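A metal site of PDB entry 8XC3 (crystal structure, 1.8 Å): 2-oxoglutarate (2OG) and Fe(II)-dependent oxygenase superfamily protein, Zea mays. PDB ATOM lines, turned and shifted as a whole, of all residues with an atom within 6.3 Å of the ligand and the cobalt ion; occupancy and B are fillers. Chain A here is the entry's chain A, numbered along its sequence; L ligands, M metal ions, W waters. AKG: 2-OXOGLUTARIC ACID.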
ATOM      1  N   GLN A 138     -21.867  16.501 -34.287  1.00  0.00           N
ATOM      2  CA  GLN A 138     -23.160  16.358 -33.621  1.00  0.00           C
ATOM      3  C   GLN A 138     -23.622  17.689 -33.080  1.00  0.00           C
ATOM      4  O   GLN A 138     -22.827  18.602 -32.814  1.00  0.00           O
ATOM      5  CB  GLN A 138     -23.121  15.336 -32.474  1.00  0.00           C
ATOM      6  CG  GLN A 138     -22.255  15.778 -31.293  1.00  0.00           C
ATOM      7  CD  GLN A 138     -23.044  15.904 -30.008  1.00  0.00           C
ATOM      8  OE1 GLN A 138     -22.992  16.940 -29.345  1.00  0.00           O
ATOM      9  NE2 GLN A 138     -23.773  14.858 -29.655  1.00  0.00           N
ATOM     10  N   ARG A 209     -29.746  14.577 -22.279  1.00  0.00           N
ATOM     11  CA  ARG A 209     -28.945  15.000 -23.418  1.00  0.00           C
ATOM     12  C   ARG A 209     -29.486  14.305 -24.655  1.00  0.00           C
ATOM     13  O   ARG A 209     -29.362  13.077 -24.796  1.00  0.00           O
ATOM     14  CB  ARG A 209     -27.452  14.698 -23.203  1.00  0.00           C
ATOM     15  CG  ARG A 209     -26.577  15.177 -24.376  1.00  0.00           C
ATOM     16  CD  ARG A 209     -25.096  14.853 -24.132  1.00  0.00           C
ATOM     17  NE  ARG A 209     -24.285  15.139 -25.313  1.00  0.00           N
ATOM     18  CZ  ARG A 209     -23.356  16.088 -25.390  1.00  0.00           C
ATOM     19  NH1 ARG A 209     -23.091  16.852 -24.344  1.00  0.00           N
ATOM     20  NH2 ARG A 209     -22.677  16.267 -26.528  1.00  0.00           N
ATOM     21  N   ASN A 211     -28.884  13.775 -28.321  1.00  0.00           N
ATOM     22  CA  ASN A 211     -27.819  13.922 -29.305  1.00  0.00           C
ATOM     23  C   ASN A 211     -28.375  13.783 -30.718  1.00  0.00           C
ATOM     24  O   ASN A 211     -29.153  12.876 -31.008  1.00  0.00           O
ATOM     25  CB  ASN A 211     -26.715  12.903 -29.108  1.00  0.00           C
ATOM     26  CG  ASN A 211     -26.015  13.069 -27.786  1.00  0.00           C
ATOM     27  OD1 ASN A 211     -25.342  14.067 -27.551  1.00  0.00           O
ATOM     28  ND2 ASN A 211     -26.178  12.087 -26.909  1.00  0.00           N
ATOM     29  N   TYR A 213     -26.789  13.307 -34.478  1.00  0.00           N
ATOM     30  CA  TYR A 213     -25.617  13.082 -35.317  1.00  0.00           C
ATOM     31  C   TYR A 213     -26.024  13.147 -36.793  1.00  0.00           C
ATOM     32  O   TYR A 213     -26.641  12.205 -37.292  1.00  0.00           O
ATOM     33  CB  TYR A 213     -24.973  11.728 -35.022  1.00  0.00           C
ATOM     34  CG  TYR A 213     -24.671  11.526 -33.550  1.00  0.00           C
ATOM     35  CD1 TYR A 213     -25.603  10.966 -32.697  1.00  0.00           C
ATOM     36  CD2 TYR A 213     -23.423  11.867 -33.025  1.00  0.00           C
ATOM     37  CE1 TYR A 213     -25.314  10.777 -31.336  1.00  0.00           C
ATOM     38  CE2 TYR A 213     -23.126  11.698 -31.670  1.00  0.00           C
ATOM     39  CZ  TYR A 213     -24.062  11.144 -30.836  1.00  0.00           C
ATOM     40  OH  TYR A 213     -23.759  10.974 -29.494  1.00  0.00           O
ATOM     41  N   ILE A 225     -19.316  11.563 -31.430  1.00  0.00           N
ATOM     42  CA  ILE A 225     -18.925  12.104 -30.138  1.00  0.00           C
ATOM     43  C   ILE A 225     -17.621  11.419 -29.764  1.00  0.00           C
ATOM     44  O   ILE A 225     -17.479  10.197 -29.929  1.00  0.00           O
ATOM     45  CB  ILE A 225     -20.045  11.929 -29.075  1.00  0.00           C
ATOM     46  CG1 ILE A 225     -19.826  12.885 -27.909  1.00  0.00           C
ATOM     47  CG2 ILE A 225     -20.192  10.515 -28.606  1.00  0.00           C
ATOM     48  CD1 ILE A 225     -21.001  12.899 -26.895  1.00  0.00           C
ATOM     49  N   HIS A 228     -14.790   9.242 -24.549  1.00  0.00           N
ATOM     50  CA  HIS A 228     -14.978   9.835 -23.230  1.00  0.00           C
ATOM     51  C   HIS A 228     -15.572   8.788 -22.311  1.00  0.00           C
ATOM     52  O   HIS A 228     -16.129   7.781 -22.758  1.00  0.00           O
ATOM     53  CB  HIS A 228     -15.903  11.055 -23.283  1.00  0.00           C
ATOM     54  CG  HIS A 228     -17.326  10.692 -23.559  1.00  0.00           C
ATOM     55  ND1 HIS A 228     -17.802  10.440 -24.832  1.00  0.00           N
ATOM     56  CD2 HIS A 228     -18.388  10.556 -22.733  1.00  0.00           C
ATOM     57  CE1 HIS A 228     -19.083  10.154 -24.777  1.00  0.00           C
ATOM     58  NE2 HIS A 228     -19.465  10.204 -23.505  1.00  0.00           N
ATOM     59  N   SER A 229     -15.463   9.044 -21.013  1.00  0.00           N
ATOM     60  CA  SER A 229     -16.276   8.395 -20.011  1.00  0.00           C
ATOM     61  C   SER A 229     -17.229   9.429 -19.438  1.00  0.00           C
ATOM     62  O   SER A 229     -16.908  10.626 -19.360  1.00  0.00           O
ATOM     63  CB  SER A 229     -15.425   7.745 -18.898  1.00  0.00           C
ATOM     64  OG  SER A 229     -14.532   8.682 -18.317  1.00  0.00           O
ATOM     65  N   ASP A 230     -18.428   8.982 -19.087  1.00  0.00           N
ATOM     66  CA  ASP A 230     -19.381   9.866 -18.440  1.00  0.00           C
ATOM     67  C   ASP A 230     -18.939  10.157 -16.998  1.00  0.00           C
ATOM     68  O   ASP A 230     -18.373   9.294 -16.316  1.00  0.00           O
ATOM     69  CB  ASP A 230     -20.785   9.243 -18.454  1.00  0.00           C
ATOM     70  CG  ASP A 230     -21.328   9.024 -19.851  1.00  0.00           C
ATOM     71  OD1 ASP A 230     -20.774   9.559 -20.823  1.00  0.00           O
ATOM     72  OD2 ASP A 230     -22.305   8.262 -19.986  1.00  0.00           O
ATOM     73  N   THR A 235     -25.485   6.232 -16.315  1.00  0.00           N
ATOM     74  CA  THR A 235     -26.129   6.767 -17.511  1.00  0.00           C
ATOM     75  C   THR A 235     -27.109   5.732 -18.036  1.00  0.00           C
ATOM     76  O   THR A 235     -26.796   4.543 -18.136  1.00  0.00           O
ATOM     77  CB  THR A 235     -25.110   7.081 -18.585  1.00  0.00           C
ATOM     78  OG1 THR A 235     -24.233   8.127 -18.129  1.00  0.00           O
ATOM     79  CG2 THR A 235     -25.805   7.560 -19.903  1.00  0.00           C
ATOM     80  N   LEU A 237     -29.191   5.096 -21.471  1.00  0.00           N
ATOM     81  CA  LEU A 237     -29.097   5.571 -22.852  1.00  0.00           C
ATOM     82  C   LEU A 237     -30.139   4.890 -23.718  1.00  0.00           C
ATOM     83  O   LEU A 237     -30.313   3.672 -23.666  1.00  0.00           O
ATOM     84  CB  LEU A 237     -27.691   5.310 -23.405  1.00  0.00           C
ATOM     85  CG  LEU A 237     -27.514   5.696 -24.886  1.00  0.00           C
ATOM     86  CD1 LEU A 237     -27.357   7.216 -25.038  1.00  0.00           C
ATOM     87  CD2 LEU A 237     -26.318   4.936 -25.491  1.00  0.00           C
ATOM     88  N   LEU A 238     -30.805   5.693 -24.553  1.00  0.00           N
ATOM     89  CA  LEU A 238     -31.789   5.203 -25.517  1.00  0.00           C
ATOM     90  C   LEU A 238     -31.338   5.642 -26.909  1.00  0.00           C
ATOM     91  O   LEU A 238     -31.080   6.827 -27.129  1.00  0.00           O
ATOM     92  CB  LEU A 238     -33.180   5.756 -25.181  1.00  0.00           C
ATOM     93  CG  LEU A 238     -34.272   5.549 -26.239  1.00  0.00           C
ATOM     94  CD1 LEU A 238     -34.460   4.062 -26.487  1.00  0.00           C
ATOM     95  CD2 LEU A 238     -35.570   6.215 -25.776  1.00  0.00           C
ATOM     96  N   VAL A 239     -31.178   4.676 -27.816  1.00  0.00           N
ATOM     97  CA  VAL A 239     -30.763   4.959 -29.191  1.00  0.00           C
ATOM     98  C   VAL A 239     -31.963   4.755 -30.105  1.00  0.00           C
ATOM     99  O   VAL A 239     -32.498   3.642 -30.171  1.00  0.00           O
ATOM    100  CB  VAL A 239     -29.612   4.037 -29.641  1.00  0.00           C
ATOM    101  CG1 VAL A 239     -29.308   4.300 -31.155  1.00  0.00           C
ATOM    102  CG2 VAL A 239     -28.409   4.234 -28.772  1.00  0.00           C
ATOM    103  N   GLY A 245     -23.451   3.015 -34.233  1.00  0.00           N
ATOM    104  CA  GLY A 245     -22.570   4.143 -34.022  1.00  0.00           C
ATOM    105  C   GLY A 245     -21.823   4.029 -32.706  1.00  0.00           C
ATOM    106  O   GLY A 245     -20.633   4.355 -32.620  1.00  0.00           O
ATOM    107  N   LEU A 246     -22.510   3.559 -31.673  1.00  0.00           N
ATOM    108  CA  LEU A 246     -21.903   3.486 -30.344  1.00  0.00           C
ATOM    109  C   LEU A 246     -20.856   2.380 -30.276  1.00  0.00           C
ATOM    110  O   LEU A 246     -21.111   1.232 -30.676  1.00  0.00           O
ATOM    111  CB  LEU A 246     -22.975   3.274 -29.292  1.00  0.00           C
ATOM    112  CG  LEU A 246     -22.404   3.218 -27.864  1.00  0.00           C
ATOM    113  CD1 LEU A 246     -21.736   4.549 -27.520  1.00  0.00           C
ATOM    114  CD2 LEU A 246     -23.507   2.932 -26.890  1.00  0.00           C
ATOM    115  N   ASN A 267     -24.687   2.412 -18.494  1.00  0.00           N
ATOM    116  CA  ASN A 267     -23.238   2.421 -18.338  1.00  0.00           C
ATOM    117  C   ASN A 267     -22.863   3.195 -17.081  1.00  0.00           C
ATOM    118  O   ASN A 267     -23.552   4.144 -16.693  1.00  0.00           O
ATOM    119  CB  ASN A 267     -22.504   3.001 -19.576  1.00  0.00           C
ATOM    120  CG  ASN A 267     -22.733   4.480 -19.785  1.00  0.00           C
ATOM    121  OD1 ASN A 267     -23.674   4.884 -20.478  1.00  0.00           O
ATOM    122  ND2 ASN A 267     -21.823   5.299 -19.254  1.00  0.00           N
ATOM    123  N   HIS A 285     -16.232   5.383 -24.147  1.00  0.00           N
ATOM    124  CA  HIS A 285     -17.089   5.092 -25.286  1.00  0.00           C
ATOM    125  C   HIS A 285     -17.061   6.249 -26.282  1.00  0.00           C
ATOM    126  O   HIS A 285     -16.598   7.364 -25.973  1.00  0.00           O
ATOM    127  CB  HIS A 285     -18.522   4.782 -24.828  1.00  0.00           C
ATOM    128  CG  HIS A 285     -19.125   5.811 -23.924  1.00  0.00           C
ATOM    129  ND1 HIS A 285     -18.850   5.864 -22.575  1.00  0.00           N
ATOM    130  CD2 HIS A 285     -19.984   6.817 -24.173  1.00  0.00           C
ATOM    131  CE1 HIS A 285     -19.537   6.856 -22.024  1.00  0.00           C
ATOM    132  NE2 HIS A 285     -20.222   7.460 -22.988  1.00  0.00           N
ATOM    133  N   ARG A 286     -17.556   5.973 -27.483  1.00  0.00           N
ATOM    134  CA  ARG A 286     -17.542   6.946 -28.582  1.00  0.00           C
ATOM    135  C   ARG A 286     -18.649   6.619 -29.555  1.00  0.00           C
ATOM    136  O   ARG A 286     -19.195   5.516 -29.572  1.00  0.00           O
ATOM    137  CB  ARG A 286     -16.191   6.975 -29.316  1.00  0.00           C
ATOM    138  CG  ARG A 286     -15.903   5.729 -30.144  1.00  0.00           C
ATOM    139  CD  ARG A 286     -14.536   5.830 -30.807  1.00  0.00           C
ATOM    140  NE  ARG A 286     -14.316   4.704 -31.722  1.00  0.00           N
ATOM    141  CZ  ARG A 286     -13.139   4.423 -32.290  1.00  0.00           C
ATOM    142  NH1 ARG A 286     -12.065   5.161 -32.057  1.00  0.00           N
ATOM    143  NH2 ARG A 286     -13.040   3.370 -33.091  1.00  0.00           N
ATOM    144  N   VAL A 287     -18.955   7.595 -30.416  1.00  0.00           N
ATOM    145  CA  VAL A 287     -19.920   7.388 -31.483  1.00  0.00           C
ATOM    146  C   VAL A 287     -19.236   7.719 -32.802  1.00  0.00           C
ATOM    147  O   VAL A 287     -18.673   8.805 -32.964  1.00  0.00           O
ATOM    148  CB  VAL A 287     -21.193   8.230 -31.274  1.00  0.00           C
ATOM    149  CG1 VAL A 287     -22.072   8.177 -32.531  1.00  0.00           C
ATOM    150  CG2 VAL A 287     -21.985   7.690 -30.085  1.00  0.00           C
ATOM    151  N   ARG A 295     -28.391  10.025 -36.831  1.00  0.00           N
ATOM    152  CA  ARG A 295     -28.517   9.163 -35.672  1.00  0.00           C
ATOM    153  C   ARG A 295     -28.974  10.010 -34.493  1.00  0.00           C
ATOM    154  O   ARG A 295     -28.461  11.128 -34.302  1.00  0.00           O
ATOM    155  CB  ARG A 295     -27.185   8.470 -35.340  1.00  0.00           C
ATOM    156  CG  ARG A 295     -27.263   7.529 -34.141  1.00  0.00           C
ATOM    157  CD  ARG A 295     -25.937   6.805 -33.965  1.00  0.00           C
ATOM    158  NE  ARG A 295     -25.994   5.895 -32.815  1.00  0.00           N
ATOM    159  CZ  ARG A 295     -25.795   6.270 -31.557  1.00  0.00           C
ATOM    160  NH1 ARG A 295     -25.531   7.547 -31.271  1.00  0.00           N
ATOM    161  NH2 ARG A 295     -25.864   5.383 -30.591  1.00  0.00           N
ATOM    162  N   LEU A 296     -29.938   9.506 -33.733  1.00  0.00           N
ATOM    163  CA  LEU A 296     -30.465  10.197 -32.561  1.00  0.00           C
ATOM    164  C   LEU A 296     -30.353   9.316 -31.316  1.00  0.00           C
ATOM    165  O   LEU A 296     -30.720   8.125 -31.338  1.00  0.00           O
ATOM    166  CB  LEU A 296     -31.936  10.609 -32.739  1.00  0.00           C
ATOM    167  CG  LEU A 296     -32.222  11.792 -33.662  1.00  0.00           C
ATOM    168  CD1 LEU A 296     -32.202  11.356 -35.098  1.00  0.00           C
ATOM    169  CD2 LEU A 296     -33.575  12.414 -33.316  1.00  0.00           C
ATOM    170  N   SER A 297     -29.888   9.905 -30.231  1.00  0.00           N
ATOM    171  CA  SER A 297     -29.881   9.224 -28.934  1.00  0.00           C
ATOM    172  C   SER A 297     -30.331  10.172 -27.833  1.00  0.00           C
ATOM    173  O   SER A 297     -30.228  11.393 -27.952  1.00  0.00           O
ATOM    174  CB  SER A 297     -28.496   8.626 -28.586  1.00  0.00           C
ATOM    175  OG  SER A 297     -27.543   9.655 -28.367  1.00  0.00           O
ATOM    176  N   LEU A 298     -30.754   9.576 -26.718  1.00  0.00           N
ATOM    177  CA  LEU A 298     -31.095  10.332 -25.518  1.00  0.00           C
ATOM    178  C   LEU A 298     -30.372   9.686 -24.341  1.00  0.00           C
ATOM    179  O   LEU A 298     -30.585   8.510 -24.044  1.00  0.00           O
ATOM    180  CB  LEU A 298     -32.610  10.355 -25.275  1.00  0.00           C
ATOM    181  CG  LEU A 298     -33.041  10.854 -23.882  1.00  0.00           C
ATOM    182  CD1 LEU A 298     -32.506  12.267 -23.590  1.00  0.00           C
ATOM    183  CD2 LEU A 298     -34.543  10.846 -23.779  1.00  0.00           C
ATOM    184  N   ALA A 299     -29.468  10.440 -23.741  1.00  0.00           N
ATOM    185  CA  ALA A 299     -28.744   9.977 -22.554  1.00  0.00           C
ATOM    186  C   ALA A 299     -29.336  10.660 -21.326  1.00  0.00           C
ATOM    187  O   ALA A 299     -29.534  11.869 -21.322  1.00  0.00           O
ATOM    188  CB  ALA A 299     -27.254  10.283 -22.674  1.00  0.00           C
ATOM    189  N   PHE A 301     -28.191  11.304 -17.694  1.00  0.00           N
ATOM    190  CA  PHE A 301     -27.034  11.283 -16.814  1.00  0.00           C
ATOM    191  C   PHE A 301     -27.504  11.463 -15.387  1.00  0.00           C
ATOM    192  O   PHE A 301     -28.102  12.498 -15.060  1.00  0.00           O
ATOM    193  CB  PHE A 301     -26.055  12.405 -17.141  1.00  0.00           C
ATOM    194  CG  PHE A 301     -25.569  12.388 -18.556  1.00  0.00           C
ATOM    195  CD1 PHE A 301     -24.902  11.294 -19.057  1.00  0.00           C
ATOM    196  CD2 PHE A 301     -25.810  13.474 -19.390  1.00  0.00           C
ATOM    197  CE1 PHE A 301     -24.462  11.277 -20.376  1.00  0.00           C
ATOM    198  CE2 PHE A 301     -25.359  13.471 -20.697  1.00  0.00           C
ATOM    199  CZ  PHE A 301     -24.698  12.357 -21.191  1.00  0.00           C
HETATM  200  C1  AKG L   1     -23.129  10.940 -24.268  1.00  0.00           C
HETATM  201  O1  AKG L   1     -23.992  11.800 -24.612  1.00  0.00           O
HETATM  202  O2  AKG L   1     -22.442  11.125 -23.247  1.00  0.00           O
HETATM  203  C2  AKG L   1     -22.926   9.687 -25.120  1.00  0.00           C
HETATM  204  O5  AKG L   1     -21.956   9.006 -24.975  1.00  0.00           O
HETATM  205  C3  AKG L   1     -23.981   9.344 -26.184  1.00  0.00           C
HETATM  206  C4  AKG L   1     -23.665   8.047 -26.936  1.00  0.00           C
HETATM  207  C5  AKG L   1     -24.668   7.729 -28.048  1.00  0.00           C
HETATM  208  O3  AKG L   1     -25.157   8.677 -28.735  1.00  0.00           O
HETATM  209  O4  AKG L   1     -25.003   6.517 -28.267  1.00  0.00           O
HETATM  210 CO    CO M   1     -21.226   9.276 -22.945  1.00  0.00          CO
HETATM  211  O   HOH W   1     -21.731  13.566 -22.912  1.00  0.00           O
HETATM  212  O   HOH W   2     -23.104   8.150 -22.338  1.00  0.00           O
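The side-chain hydroxyl of Ser 297 is in hydrogen-bond range of an oxygen (O3) of the ligand, 2.6 Å away.
NE of Arg 209 is in salt-bridge range of O1 of the ligand (3.4 Å).
The guanidinium group (NH2) of Arg 295 lies within salt-bridge range of an oxygen (O4) of the ligand (2.7 Å).
O3 of the ligand sits at hydrogen-bond distance from OH of Tyr 213, 2.8 Å away.
The side-chain amide nitrogen (ND2) of Asn 211 lies within hydrogen-bond range of an oxygen (O1) of the ligand, at 3.2 Å.
The side-chain carboxylate of Asp 230 sits at hydrogen-bond distance from the side-chain amide nitrogen of Asn 267 (3.1 Å).
O of Arg 209 is in hydrogen-bond range of N of Ala 299, at 2.8 Å.
OD1 of Asn 211 sits at hydrogen-bond distance from NE2 of Gln 138, 2.7 Å away.
OD2 of Asp 230 lies within hydrogen-bond range of OG1 of Thr 235, at 2.7 Å.
N of Tyr 213 lies within hydrogen-bond range of O of Arg 295, 2.8 Å away.
O of Ile 225 sits at hydrogen-bond distance from N of Val 287.
NE of Arg 209 is in hydrogen-bond range of OD1 of Asn 211 (2.7 Å).
The guanidinium group of Arg 209 lies within hydrogen-bond range of the side-chain amide oxygen of Gln 138, at 2.9 Å.
Merely in contact with the ligand: Phe 301 (3.3 Å), Val 287 (3.4 Å), Leu 237 (3.5 Å), Leu 246 (3.9 Å) and Ile 225 (3.9 Å).
Hydrophobic or aromatic side chains that line the ligand: Tyr 213, Ile 225, His 228, Leu 237, Leu 246, His 285, Val 287 and Phe 301.
Within 4 Å of the ligand: Arg 209, Asn 211, Tyr 213, Ile 225, His 228, Asp 230, Leu 237, Leu 246, His 285, Val 287, Arg 295, Ser 297 and Phe 301.
Three residues have an atom within 4 Å of the cobalt ion: His 228, Asp 230 and His 285.
The nearest printed residue that does not touch the cobalt ion is Phe 301 (4.6 Å).
The cobalt ion is bound by NE2 of His 228 (2.1 Å), NE2 of His 285 (2.1 Å), O5 of the ligand (2.2 Å), OD1 of Asp 230 (2.2 Å), O2 of the ligand (2.2 Å) and water W2 (2.3 Å).
The cobalt ion has six donor atoms within binding distance.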
